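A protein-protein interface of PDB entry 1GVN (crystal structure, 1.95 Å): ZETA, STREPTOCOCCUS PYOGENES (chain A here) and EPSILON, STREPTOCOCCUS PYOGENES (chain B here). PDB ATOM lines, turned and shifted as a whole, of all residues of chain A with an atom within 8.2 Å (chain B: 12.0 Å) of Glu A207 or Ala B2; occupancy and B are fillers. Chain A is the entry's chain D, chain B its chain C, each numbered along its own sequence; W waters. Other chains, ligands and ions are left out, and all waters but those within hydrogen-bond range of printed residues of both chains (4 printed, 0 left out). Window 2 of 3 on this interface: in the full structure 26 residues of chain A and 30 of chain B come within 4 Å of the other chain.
The backbone carbonyl oxygen (O) of Glu A207 lies within hydrogen-bond range of the backbone NH (N) of Ala B2 (3.3 Å). The backbone NH (N) of Val B3 lies within hydrogen-bond range of the backbone carbonyl oxygen (O) of Glu A207.
Printed residues of chain B that touch a printed residue of chain A: Ala B2, Val B3, Tyr B5, Thr B8 and Phe B59. Hydrophobic or aromatic side chains of chain B that line the printed part of chain A: Val B3, Tyr B5 and Phe B59. Along chain B the printed residues that touch a printed residue of chain A span positions 2 to 59. Of the 20 printed residues of chain A, 4 touch a printed residue of chain B. Printed residues of chain A that touch a printed residue of chain B: Ser A48, Ser A51, Arg A206 and Glu A207. Along chain A the printed residues that touch a printed residue of chain B span positions 48 to 207. Among the printed residues, 7 pairs touch across the chains. Among the printed residues, no Asp or Glu carboxylate lies within 4 Å of a Lys or Arg side-chain nitrogen of the other chain.
Among the printed residues, merely in contact across the chains: Ser A48 with Thr B8 (3.5 Å), Ser A51 with Val B3 (3.5 Å), Ser A51 with Phe B59 (3.6 Å), Arg A206 with Val B3 (3.5 Å) and Arg A206 with Tyr B5 (3.3 Å).
Of the printed residues of chain B, Glu A207 touches Ala B2 (3.3 Å) and Val B3 (3.2 Å). Ala B2 touches one residue of chain A. Ser A48 touches one residue of chain B. No residue of chain B comes within 4 Å of Val A209. Printed residues of chain B within 4 Å of Arg A206: Val B3 (3.5 Å) and Tyr B5 (3.3 Å). Of the printed residues of chain A, Val B3 touches Ser A51 (3.5 Å), Arg A206 (3.5 Å) and Glu A207 (3.2 Å). Leu A211 touches none of the printed residues of chain B. Ile B11 touches none of the printed residues of chain A. The nearest residue of chain B that does not touch Glu A207 is Tyr B5 (4.4 Å).
The side-chain hydroxyl (OG) of Ser A48 lies within hydrogen-bond range of the backbone carbonyl oxygen (O) of Gly A45, 3.3 Å away. O of Ser A48 is in hydrogen-bond range of OG of Ser A51 (2.5 Å). The side-chain hydroxyl of Ser A48 lies within hydrogen-bond range of the backbone carbonyl oxygen of Arg A206. OG1 of Thr B8 sits at hydrogen-bond distance from O of Thr B4 (2.9 Å). OD1 of Asn B57 lies close to N of Phe B59, at 3.1 Å. O of Tyr B5 lies within hydrogen-bond range of OG1 of Thr B8.
Water W1 lies within hydrogen-bond range of the side-chain hydroxyl (OG1) of Thr B8 (2.7 Å), the side-chain hydroxyl (OG) of Ser A48 (3.0 Å) and the backbone carbonyl oxygen (O) of Gly A45 (3.1 Å). Water W4 lies within hydrogen-bond range of OG of Ser A51 and N of Ala B2. Water W3 lies within hydrogen-bond range of N of Tyr B5 and OE2 of Glu A207. Water W2 bridges the backbone NH of Ala B2 (3.1 Å) and the side-chain carboxylate of Glu A55 (3.2 Å).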
ATOM      1  N   SER A  44     -12.548 -22.622 -37.836  1.00  0.00           N
ATOM      2  CA  SER A  44     -13.237 -23.815 -37.338  1.00  0.00           C
ATOM      3  C   SER A  44     -14.148 -23.525 -36.143  1.00  0.00           C
ATOM      4  O   SER A  44     -15.196 -24.153 -36.000  1.00  0.00           O
ATOM      5  CB  SER A  44     -12.233 -24.931 -36.988  1.00  0.00           C
ATOM      6  OG  SER A  44     -11.261 -24.515 -36.043  1.00  0.00           O
ATOM      7  N   GLY A  45     -13.754 -22.573 -35.299  1.00  0.00           N
ATOM      8  CA  GLY A  45     -14.562 -22.226 -34.137  1.00  0.00           C
ATOM      9  C   GLY A  45     -14.017 -22.793 -32.837  1.00  0.00           C
ATOM     10  O   GLY A  45     -14.765 -23.333 -32.019  1.00  0.00           O
ATOM     11  N   SER A  48     -15.416 -23.084 -29.208  1.00  0.00           N
ATOM     12  CA  SER A  48     -16.257 -24.183 -28.727  1.00  0.00           C
ATOM     13  C   SER A  48     -15.431 -25.095 -27.822  1.00  0.00           C
ATOM     14  O   SER A  48     -15.951 -25.685 -26.879  1.00  0.00           O
ATOM     15  CB  SER A  48     -16.818 -24.988 -29.906  1.00  0.00           C
ATOM     16  OG  SER A  48     -17.689 -24.190 -30.696  1.00  0.00           O
ATOM     17  N   LEU A  49     -14.139 -25.206 -28.112  1.00  0.00           N
ATOM     18  CA  LEU A  49     -13.243 -26.028 -27.299  1.00  0.00           C
ATOM     19  C   LEU A  49     -13.063 -25.362 -25.936  1.00  0.00           C
ATOM     20  O   LEU A  49     -12.981 -26.035 -24.901  1.00  0.00           O
ATOM     21  CB  LEU A  49     -11.875 -26.162 -27.972  1.00  0.00           C
ATOM     22  CG  LEU A  49     -11.803 -26.740 -29.388  1.00  0.00           C
ATOM     23  CD1 LEU A  49     -10.382 -26.586 -29.916  1.00  0.00           C
ATOM     24  CD2 LEU A  49     -12.221 -28.209 -29.387  1.00  0.00           C
ATOM     25  N   SER A  51     -15.208 -23.656 -24.361  1.00  0.00           N
ATOM     26  CA  SER A  51     -16.412 -23.917 -23.577  1.00  0.00           C
ATOM     27  C   SER A  51     -16.352 -25.293 -22.935  1.00  0.00           C
ATOM     28  O   SER A  51     -16.650 -25.445 -21.752  1.00  0.00           O
ATOM     29  CB  SER A  51     -17.668 -23.826 -24.449  1.00  0.00           C
ATOM     30  OG  SER A  51     -17.791 -24.969 -25.281  1.00  0.00           O
ATOM     31  N   ALA A  52     -15.966 -26.295 -23.720  1.00  0.00           N
ATOM     32  CA  ALA A  52     -15.883 -27.659 -23.212  1.00  0.00           C
ATOM     33  C   ALA A  52     -14.871 -27.784 -22.078  1.00  0.00           C
ATOM     34  O   ALA A  52     -15.105 -28.502 -21.103  1.00  0.00           O
ATOM     35  CB  ALA A  52     -15.526 -28.617 -24.341  1.00  0.00           C
ATOM     36  N   GLU A  55     -15.975 -26.061 -18.863  1.00  0.00           N
ATOM     37  CA  GLU A  55     -16.916 -26.954 -18.196  1.00  0.00           C
ATOM     38  C   GLU A  55     -16.172 -28.046 -17.437  1.00  0.00           C
ATOM     39  O   GLU A  55     -16.441 -28.294 -16.260  1.00  0.00           O
ATOM     40  CB  GLU A  55     -17.849 -27.583 -19.231  1.00  0.00           C
ATOM     41  CG  GLU A  55     -18.987 -28.402 -18.653  1.00  0.00           C
ATOM     42  CD  GLU A  55     -19.871 -28.994 -19.739  1.00  0.00           C
ATOM     43  OE1 GLU A  55     -19.452 -29.982 -20.386  1.00  0.00           O
ATOM     44  OE2 GLU A  55     -20.980 -28.462 -19.956  1.00  0.00           O
ATOM     45  N   MET A 144     -10.736 -28.949 -33.088  1.00  0.00           N
ATOM     46  CA  MET A 144     -11.984 -28.816 -33.821  1.00  0.00           C
ATOM     47  C   MET A 144     -11.918 -29.703 -35.062  1.00  0.00           C
ATOM     48  O   MET A 144     -10.872 -29.811 -35.707  1.00  0.00           O
ATOM     49  CB  MET A 144     -12.210 -27.366 -34.269  1.00  0.00           C
ATOM     50  CG  MET A 144     -12.511 -26.388 -33.149  1.00  0.00           C
ATOM     51  SD  MET A 144     -13.936 -26.873 -32.171  1.00  0.00           S
ATOM     52  CE  MET A 144     -15.283 -26.693 -33.361  1.00  0.00           C
ATOM     53  N   ALA A 145     -13.038 -30.341 -35.376  1.00  0.00           N
ATOM     54  CA  ALA A 145     -13.163 -31.187 -36.554  1.00  0.00           C
ATOM     55  C   ALA A 145     -14.353 -30.564 -37.263  1.00  0.00           C
ATOM     56  O   ALA A 145     -15.505 -30.816 -36.904  1.00  0.00           O
ATOM     57  CB  ALA A 145     -13.471 -32.627 -36.151  1.00  0.00           C
ATOM     58  N   VAL A 146     -14.063 -29.731 -38.258  1.00  0.00           N
ATOM     59  CA  VAL A 146     -15.098 -29.012 -38.993  1.00  0.00           C
ATOM     60  C   VAL A 146     -14.854 -29.057 -40.499  1.00  0.00           C
ATOM     61  O   VAL A 146     -13.711 -28.988 -40.953  1.00  0.00           O
ATOM     62  CB  VAL A 146     -15.132 -27.537 -38.524  1.00  0.00           C
ATOM     63  CG1 VAL A 146     -16.170 -26.738 -39.305  1.00  0.00           C
ATOM     64  CG2 VAL A 146     -15.430 -27.488 -37.029  1.00  0.00           C
ATOM     65  N   TYR A 204     -13.788 -32.232 -31.626  1.00  0.00           N
ATOM     66  CA  TYR A 204     -15.094 -31.669 -31.277  1.00  0.00           C
ATOM     67  C   TYR A 204     -15.711 -30.957 -32.470  1.00  0.00           C
ATOM     68  O   TYR A 204     -14.993 -30.497 -33.359  1.00  0.00           O
ATOM     69  CB  TYR A 204     -14.942 -30.620 -30.171  1.00  0.00           C
ATOM     70  CG  TYR A 204     -14.815 -31.149 -28.766  1.00  0.00           C
ATOM     71  CD1 TYR A 204     -15.946 -31.385 -27.985  1.00  0.00           C
ATOM     72  CD2 TYR A 204     -13.564 -31.396 -28.208  1.00  0.00           C
ATOM     73  CE1 TYR A 204     -15.832 -31.854 -26.677  1.00  0.00           C
ATOM     74  CE2 TYR A 204     -13.437 -31.862 -26.903  1.00  0.00           C
ATOM     75  CZ  TYR A 204     -14.571 -32.088 -26.144  1.00  0.00           C
ATOM     76  OH  TYR A 204     -14.438 -32.525 -24.848  1.00  0.00           O
ATOM     77  N   ASN A 205     -17.039 -30.865 -32.498  1.00  0.00           N
ATOM     78  CA  ASN A 205     -17.687 -30.119 -33.569  1.00  0.00           C
ATOM     79  C   ASN A 205     -18.089 -28.785 -32.937  1.00  0.00           C
ATOM     80  O   ASN A 205     -17.845 -28.569 -31.749  1.00  0.00           O
ATOM     81  CB  ASN A 205     -18.904 -30.863 -34.136  1.00  0.00           C
ATOM     82  CG  ASN A 205     -20.010 -31.056 -33.122  1.00  0.00           C
ATOM     83  OD1 ASN A 205     -20.066 -30.374 -32.090  1.00  0.00           O
ATOM     84  ND2 ASN A 205     -20.917 -31.977 -33.421  1.00  0.00           N
ATOM     85  N   ARG A 206     -18.696 -27.893 -33.711  1.00  0.00           N
ATOM     86  CA  ARG A 206     -19.070 -26.580 -33.189  1.00  0.00           C
ATOM     87  C   ARG A 206     -20.053 -26.548 -32.021  1.00  0.00           C
ATOM     88  O   ARG A 206     -20.084 -25.569 -31.267  1.00  0.00           O
ATOM     89  CB  ARG A 206     -19.588 -25.699 -34.328  1.00  0.00           C
ATOM     90  CG  ARG A 206     -18.487 -25.281 -35.292  1.00  0.00           C
ATOM     91  CD  ARG A 206     -19.034 -24.618 -36.546  1.00  0.00           C
ATOM     92  NE  ARG A 206     -17.958 -24.014 -37.326  1.00  0.00           N
ATOM     93  CZ  ARG A 206     -18.139 -23.356 -38.467  1.00  0.00           C
ATOM     94  NH1 ARG A 206     -19.356 -23.217 -38.971  1.00  0.00           N
ATOM     95  NH2 ARG A 206     -17.100 -22.820 -39.092  1.00  0.00           N
ATOM     96  N   GLU A 207     -20.853 -27.599 -31.861  1.00  0.00           N
ATOM     97  CA  GLU A 207     -21.810 -27.636 -30.757  1.00  0.00           C
ATOM     98  C   GLU A 207     -21.204 -28.252 -29.503  1.00  0.00           C
ATOM     99  O   GLU A 207     -21.922 -28.571 -28.555  1.00  0.00           O
ATOM    100  CB  GLU A 207     -23.068 -28.424 -31.139  1.00  0.00           C
ATOM    101  CG  GLU A 207     -23.913 -27.787 -32.227  1.00  0.00           C
ATOM    102  CD  GLU A 207     -23.213 -27.770 -33.565  1.00  0.00           C
ATOM    103  OE1 GLU A 207     -22.732 -28.842 -33.994  1.00  0.00           O
ATOM    104  OE2 GLU A 207     -23.147 -26.693 -34.191  1.00  0.00           O
ATOM    105  N   GLY A 208     -19.884 -28.417 -29.496  1.00  0.00           N
ATOM    106  CA  GLY A 208     -19.224 -28.990 -28.338  1.00  0.00           C
ATOM    107  C   GLY A 208     -19.402 -30.491 -28.186  1.00  0.00           C
ATOM    108  O   GLY A 208     -19.202 -31.036 -27.103  1.00  0.00           O
ATOM    109  N   VAL A 209     -19.777 -31.167 -29.265  1.00  0.00           N
ATOM    110  CA  VAL A 209     -19.964 -32.614 -29.229  1.00  0.00           C
ATOM    111  C   VAL A 209     -18.628 -33.326 -29.440  1.00  0.00           C
ATOM    112  O   VAL A 209     -17.929 -33.058 -30.416  1.00  0.00           O
ATOM    113  CB  VAL A 209     -20.933 -33.077 -30.332  1.00  0.00           C
ATOM    114  CG1 VAL A 209     -21.026 -34.597 -30.333  1.00  0.00           C
ATOM    115  CG2 VAL A 209     -22.307 -32.448 -30.121  1.00  0.00           C
ATOM    116  N   LYS A 210     -18.282 -34.228 -28.524  1.00  0.00           N
ATOM    117  CA  LYS A 210     -17.034 -34.985 -28.617  1.00  0.00           C
ATOM    118  C   LYS A 210     -17.172 -36.066 -29.686  1.00  0.00           C
ATOM    119  O   LYS A 210     -17.988 -36.973 -29.559  1.00  0.00           O
ATOM    120  CB  LYS A 210     -16.704 -35.622 -27.263  1.00  0.00           C
ATOM    121  CG  LYS A 210     -15.394 -36.400 -27.246  1.00  0.00           C
ATOM    122  CD  LYS A 210     -15.005 -36.833 -25.832  1.00  0.00           C
ATOM    123  CE  LYS A 210     -16.083 -37.692 -25.181  1.00  0.00           C
ATOM    124  NZ  LYS A 210     -16.437 -38.868 -26.020  1.00  0.00           N
ATOM    125  N   LEU A 211     -16.364 -35.966 -30.734  1.00  0.00           N
ATOM    126  CA  LEU A 211     -16.413 -36.907 -31.848  1.00  0.00           C
ATOM    127  C   LEU A 211     -15.336 -37.984 -31.798  1.00  0.00           C
ATOM    128  O   LEU A 211     -15.434 -39.004 -32.481  1.00  0.00           O
ATOM    129  CB  LEU A 211     -16.276 -36.144 -33.165  1.00  0.00           C
ATOM    130  CG  LEU A 211     -17.268 -35.003 -33.400  1.00  0.00           C
ATOM    131  CD1 LEU A 211     -16.861 -34.212 -34.631  1.00  0.00           C
ATOM    132  CD2 LEU A 211     -18.670 -35.572 -33.560  1.00  0.00           C
ATOM    133  N   ARG A 232     -16.156 -33.647 -45.551  1.00  0.00           N
ATOM    134  CA  ARG A 232     -17.579 -33.942 -45.626  1.00  0.00           C
ATOM    135  C   ARG A 232     -18.305 -32.935 -46.520  1.00  0.00           C
ATOM    136  O   ARG A 232     -18.092 -31.727 -46.406  1.00  0.00           O
ATOM    137  CB  ARG A 232     -18.181 -33.920 -44.225  1.00  0.00           C
ATOM    138  CG  ARG A 232     -19.515 -34.614 -44.130  1.00  0.00           C
ATOM    139  CD  ARG A 232     -20.539 -33.695 -43.531  1.00  0.00           C
ATOM    140  NE  ARG A 232     -20.155 -33.234 -42.203  1.00  0.00           N
ATOM    141  CZ  ARG A 232     -20.766 -32.241 -41.566  1.00  0.00           C
ATOM    142  NH1 ARG A 232     -21.783 -31.617 -42.145  1.00  0.00           N
ATOM    143  NH2 ARG A 232     -20.362 -31.872 -40.360  1.00  0.00           N
ATOM    144  N   GLU A 238     -27.884 -26.870 -45.261  1.00  0.00           N
ATOM    145  CA  GLU A 238     -27.058 -26.501 -44.114  1.00  0.00           C
ATOM    146  C   GLU A 238     -26.215 -25.260 -44.381  1.00  0.00           C
ATOM    147  O   GLU A 238     -25.968 -24.461 -43.479  1.00  0.00           O
ATOM    148  CB  GLU A 238     -26.119 -27.655 -43.735  1.00  0.00           C
ATOM    149  CG  GLU A 238     -25.300 -27.388 -42.474  1.00  0.00           C
ATOM    150  CD  GLU A 238     -24.175 -28.388 -42.259  1.00  0.00           C
ATOM    151  OE1 GLU A 238     -24.418 -29.610 -42.369  1.00  0.00           O
ATOM    152  OE2 GLU A 238     -23.042 -27.948 -41.964  1.00  0.00           O
ATOM    153  N   ALA B   2     -22.157 -28.427 -25.255  1.00  0.00           N
ATOM    154  CA  ALA B   2     -23.530 -27.874 -25.071  1.00  0.00           C
ATOM    155  C   ALA B   2     -23.561 -26.385 -25.412  1.00  0.00           C
ATOM    156  O   ALA B   2     -23.981 -25.562 -24.595  1.00  0.00           O
ATOM    157  CB  ALA B   2     -23.985 -28.094 -23.627  1.00  0.00           C
ATOM    158  N   VAL B   3     -23.110 -26.046 -26.617  1.00  0.00           N
ATOM    159  CA  VAL B   3     -23.078 -24.657 -27.074  1.00  0.00           C
ATOM    160  C   VAL B   3     -23.540 -24.562 -28.525  1.00  0.00           C
ATOM    161  O   VAL B   3     -23.657 -25.583 -29.213  1.00  0.00           O
ATOM    162  CB  VAL B   3     -21.650 -24.067 -26.984  1.00  0.00           C
ATOM    163  CG1 VAL B   3     -21.144 -24.145 -25.557  1.00  0.00           C
ATOM    164  CG2 VAL B   3     -20.716 -24.815 -27.921  1.00  0.00           C
ATOM    165  N   THR B   4     -23.808 -23.342 -28.986  1.00  0.00           N
ATOM    166  CA  THR B   4     -24.235 -23.134 -30.368  1.00  0.00           C
ATOM    167  C   THR B   4     -23.150 -22.379 -31.122  1.00  0.00           C
ATOM    168  O   THR B   4     -22.362 -21.640 -30.528  1.00  0.00           O
ATOM    169  CB  THR B   4     -25.553 -22.314 -30.470  1.00  0.00           C
ATOM    170  OG1 THR B   4     -25.307 -20.947 -30.115  1.00  0.00           O
ATOM    171  CG2 THR B   4     -26.613 -22.892 -29.555  1.00  0.00           C
ATOM    172  N   TYR B   5     -23.104 -22.568 -32.435  1.00  0.00           N
ATOM    173  CA  TYR B   5     -22.104 -21.890 -33.238  1.00  0.00           C
ATOM    174  C   TYR B   5     -22.340 -20.386 -33.207  1.00  0.00           C
ATOM    175  O   TYR B   5     -21.401 -19.601 -33.099  1.00  0.00           O
ATOM    176  CB  TYR B   5     -22.145 -22.387 -34.684  1.00  0.00           C
ATOM    177  CG  TYR B   5     -21.186 -21.650 -35.588  1.00  0.00           C
ATOM    178  CD1 TYR B   5     -19.816 -21.642 -35.326  1.00  0.00           C
ATOM    179  CD2 TYR B   5     -21.646 -20.963 -36.707  1.00  0.00           C
ATOM    180  CE1 TYR B   5     -18.926 -20.967 -36.160  1.00  0.00           C
ATOM    181  CE2 TYR B   5     -20.764 -20.284 -37.550  1.00  0.00           C
ATOM    182  CZ  TYR B   5     -19.409 -20.290 -37.271  1.00  0.00           C
ATOM    183  OH  TYR B   5     -18.538 -19.628 -38.108  1.00  0.00           O
ATOM    184  N   GLU B   6     -23.601 -19.986 -33.295  1.00  0.00           N
ATOM    185  CA  GLU B   6     -23.930 -18.570 -33.280  1.00  0.00           C
ATOM    186  C   GLU B   6     -23.403 -17.870 -32.028  1.00  0.00           C
ATOM    187  O   GLU B   6     -22.851 -16.771 -32.110  1.00  0.00           O
ATOM    188  CB  GLU B   6     -25.442 -18.383 -33.390  1.00  0.00           C
ATOM    189  CG  GLU B   6     -25.897 -16.945 -33.213  1.00  0.00           C
ATOM    190  CD  GLU B   6     -27.383 -16.778 -33.473  1.00  0.00           C
ATOM    191  OE1 GLU B   6     -28.167 -17.637 -33.011  1.00  0.00           O
ATOM    192  OE2 GLU B   6     -27.761 -15.787 -34.128  1.00  0.00           O
ATOM    193  N   LYS B   7     -23.557 -18.499 -30.869  1.00  0.00           N
ATOM    194  CA  LYS B   7     -23.082 -17.883 -29.638  1.00  0.00           C
ATOM    195  C   LYS B   7     -21.564 -17.955 -29.499  1.00  0.00           C
ATOM    196  O   LYS B   7     -20.935 -16.988 -29.069  1.00  0.00           O
ATOM    197  CB  LYS B   7     -23.768 -18.519 -28.423  1.00  0.00           C
ATOM    198  CG  LYS B   7     -25.257 -18.159 -28.325  1.00  0.00           C
ATOM    199  CD  LYS B   7     -25.987 -18.956 -27.248  1.00  0.00           C
ATOM    200  CE  LYS B   7     -25.430 -18.685 -25.861  1.00  0.00           C
ATOM    201  NZ  LYS B   7     -26.194 -19.418 -24.803  1.00  0.00           N
ATOM    202  N   THR B   8     -20.965 -19.086 -29.867  1.00  0.00           N
ATOM    203  CA  THR B   8     -19.515 -19.202 -29.757  1.00  0.00           C
ATOM    204  C   THR B   8     -18.830 -18.264 -30.756  1.00  0.00           C
ATOM    205  O   THR B   8     -17.702 -17.818 -30.532  1.00  0.00           O
ATOM    206  CB  THR B   8     -19.034 -20.676 -29.948  1.00  0.00           C
ATOM    207  OG1 THR B   8     -19.569 -21.222 -31.156  1.00  0.00           O
ATOM    208  CG2 THR B   8     -19.489 -21.535 -28.775  1.00  0.00           C
ATOM    209  N   PHE B   9     -19.511 -17.954 -31.854  1.00  0.00           N
ATOM    210  CA  PHE B   9     -18.958 -17.032 -32.841  1.00  0.00           C
ATOM    211  C   PHE B   9     -18.996 -15.620 -32.241  1.00  0.00           C
ATOM    212  O   PHE B   9     -18.051 -14.841 -32.399  1.00  0.00           O
ATOM    213  CB  PHE B   9     -19.766 -17.079 -34.145  1.00  0.00           C
ATOM    214  CG  PHE B   9     -19.269 -16.124 -35.199  1.00  0.00           C
ATOM    215  CD1 PHE B   9     -19.675 -14.795 -35.199  1.00  0.00           C
ATOM    216  CD2 PHE B   9     -18.373 -16.552 -36.178  1.00  0.00           C
ATOM    217  CE1 PHE B   9     -19.199 -13.896 -36.156  1.00  0.00           C
ATOM    218  CE2 PHE B   9     -17.886 -15.661 -37.144  1.00  0.00           C
ATOM    219  CZ  PHE B   9     -18.303 -14.331 -37.130  1.00  0.00           C
ATOM    220  N   ILE B  11     -18.873 -14.897 -29.144  1.00  0.00           N
ATOM    221  CA  ILE B  11     -17.861 -14.868 -28.101  1.00  0.00           C
ATOM    222  C   ILE B  11     -16.459 -14.646 -28.678  1.00  0.00           C
ATOM    223  O   ILE B  11     -15.659 -13.912 -28.104  1.00  0.00           O
ATOM    224  CB  ILE B  11     -17.911 -16.169 -27.277  1.00  0.00           C
ATOM    225  CG1 ILE B  11     -19.223 -16.205 -26.472  1.00  0.00           C
ATOM    226  CG2 ILE B  11     -16.699 -16.263 -26.357  1.00  0.00           C
ATOM    227  CD1 ILE B  11     -19.475 -17.514 -25.743  1.00  0.00           C
ATOM    228  N   ASN B  57     -17.927 -14.372 -17.336  1.00  0.00           N
ATOM    229  CA  ASN B  57     -17.795 -15.643 -18.042  1.00  0.00           C
ATOM    230  C   ASN B  57     -18.825 -15.624 -19.161  1.00  0.00           C
ATOM    231  O   ASN B  57     -20.015 -15.820 -18.923  1.00  0.00           O
ATOM    232  CB  ASN B  57     -18.045 -16.820 -17.093  1.00  0.00           C
ATOM    233  CG  ASN B  57     -18.326 -18.115 -17.828  1.00  0.00           C
ATOM    234  OD1 ASN B  57     -17.717 -18.402 -18.854  1.00  0.00           O
ATOM    235  ND2 ASN B  57     -19.250 -18.912 -17.297  1.00  0.00           N
ATOM    236  N   LEU B  58     -18.359 -15.377 -20.381  1.00  0.00           N
ATOM    237  CA  LEU B  58     -19.244 -15.302 -21.540  1.00  0.00           C
ATOM    238  C   LEU B  58     -19.979 -16.602 -21.858  1.00  0.00           C
ATOM    239  O   LEU B  58     -20.967 -16.591 -22.588  1.00  0.00           O
ATOM    240  CB  LEU B  58     -18.454 -14.850 -22.772  1.00  0.00           C
ATOM    241  CG  LEU B  58     -17.787 -13.474 -22.676  1.00  0.00           C
ATOM    242  CD1 LEU B  58     -16.977 -13.221 -23.949  1.00  0.00           C
ATOM    243  CD2 LEU B  58     -18.852 -12.383 -22.487  1.00  0.00           C
ATOM    244  N   PHE B  59     -19.504 -17.723 -21.324  1.00  0.00           N
ATOM    245  CA  PHE B  59     -20.167 -18.991 -21.597  1.00  0.00           C
ATOM    246  C   PHE B  59     -21.460 -19.131 -20.805  1.00  0.00           C
ATOM    247  O   PHE B  59     -22.236 -20.060 -21.027  1.00  0.00           O
ATOM    248  CB  PHE B  59     -19.220 -20.152 -21.302  1.00  0.00           C
ATOM    249  CG  PHE B  59     -18.018 -20.178 -22.203  1.00  0.00           C
ATOM    250  CD1 PHE B  59     -18.178 -20.216 -23.588  1.00  0.00           C
ATOM    251  CD2 PHE B  59     -16.731 -20.139 -21.675  1.00  0.00           C
ATOM    252  CE1 PHE B  59     -17.073 -20.213 -24.439  1.00  0.00           C
ATOM    253  CE2 PHE B  59     -15.616 -20.137 -22.517  1.00  0.00           C
ATOM    254  CZ  PHE B  59     -15.787 -20.172 -23.903  1.00  0.00           C
ATOM    255  N   ASP B  60     -21.700 -18.185 -19.902  1.00  0.00           N
ATOM    256  CA  ASP B  60     -22.908 -18.216 -19.086  1.00  0.00           C
ATOM    257  C   ASP B  60     -23.874 -17.092 -19.472  1.00  0.00           C
ATOM    258  O   ASP B  60     -24.607 -16.572 -18.631  1.00  0.00           O
ATOM    259  CB  ASP B  60     -22.527 -18.119 -17.606  1.00  0.00           C
ATOM    260  CG  ASP B  60     -23.727 -18.216 -16.680  1.00  0.00           C
ATOM    261  OD1 ASP B  60     -24.602 -19.074 -16.917  1.00  0.00           O
ATOM    262  OD2 ASP B  60     -23.784 -17.437 -15.704  1.00  0.00           O
ATOM    263  N   TYR B  61     -23.866 -16.711 -20.746  1.00  0.00           N
ATOM    264  CA  TYR B  61     -24.759 -15.661 -21.230  1.00  0.00           C
ATOM    265  C   TYR B  61     -25.633 -16.167 -22.368  1.00  0.00           C
ATOM    266  O   TYR B  61     -25.224 -17.025 -23.145  1.00  0.00           O
ATOM    267  CB  TYR B  61     -23.980 -14.440 -21.736  1.00  0.00           C
ATOM    268  CG  TYR B  61     -23.383 -13.553 -20.660  1.00  0.00           C
ATOM    269  CD1 TYR B  61     -24.026 -13.363 -19.439  1.00  0.00           C
ATOM    270  CD2 TYR B  61     -22.192 -12.864 -20.889  1.00  0.00           C
ATOM    271  CE1 TYR B  61     -23.496 -12.506 -18.470  1.00  0.00           C
ATOM    272  CE2 TYR B  61     -21.657 -12.011 -19.932  1.00  0.00           C
ATOM    273  CZ  TYR B  61     -22.312 -11.834 -18.726  1.00  0.00           C
ATOM    274  OH  TYR B  61     -21.773 -10.991 -17.780  1.00  0.00           O
ATOM    275  N   SER B  62     -26.842 -15.630 -22.456  1.00  0.00           N
ATOM    276  CA  SER B  62     -27.757 -16.014 -23.517  1.00  0.00           C
ATOM    277  C   SER B  62     -27.303 -15.292 -24.770  1.00  0.00           C
ATOM    278  O   SER B  62     -26.443 -14.410 -24.715  1.00  0.00           O
ATOM    279  CB  SER B  62     -29.173 -15.562 -23.184  1.00  0.00           C
ATOM    280  OG  SER B  62     -29.223 -14.146 -23.159  1.00  0.00           O
ATOM    281  N   LEU B  63     -27.896 -15.656 -25.899  1.00  0.00           N
ATOM    282  CA  LEU B  63     -27.561 -15.028 -27.168  1.00  0.00           C
ATOM    283  C   LEU B  63     -27.790 -13.518 -27.091  1.00  0.00           C
ATOM    284  O   LEU B  63     -26.942 -12.728 -27.508  1.00  0.00           O
ATOM    285  CB  LEU B  63     -28.419 -15.627 -28.285  1.00  0.00           C
ATOM    286  CG  LEU B  63     -28.337 -14.967 -29.665  1.00  0.00           C
ATOM    287  CD1 LEU B  63     -26.900 -15.042 -30.193  1.00  0.00           C
ATOM    288  CD2 LEU B  63     -29.306 -15.662 -30.619  1.00  0.00           C
ATOM    289  N   LEU B  66     -25.155 -11.851 -25.090  1.00  0.00           N
ATOM    290  CA  LEU B  66     -23.891 -11.814 -25.820  1.00  0.00           C
ATOM    291  C   LEU B  66     -23.911 -10.679 -26.838  1.00  0.00           C
ATOM    292  O   LEU B  66     -22.922  -9.961 -27.005  1.00  0.00           O
ATOM    293  CB  LEU B  66     -23.619 -13.153 -26.525  1.00  0.00           C
ATOM    294  CG  LEU B  66     -23.236 -14.333 -25.620  1.00  0.00           C
ATOM    295  CD1 LEU B  66     -22.973 -15.573 -26.469  1.00  0.00           C
ATOM    296  CD2 LEU B  66     -21.998 -13.981 -24.812  1.00  0.00           C
HETATM  297  O   HOH W   1     -17.462 -21.984 -32.657  1.00  0.00           O
HETATM  298  O   HOH W   2     -21.101 -26.957 -22.755  1.00  0.00           O
HETATM  299  O   HOH W   3     -24.798 -24.530 -33.493  1.00  0.00           O
HETATM  300  O   HOH W   4     -19.358 -27.193 -24.661  1.00  0.00           O
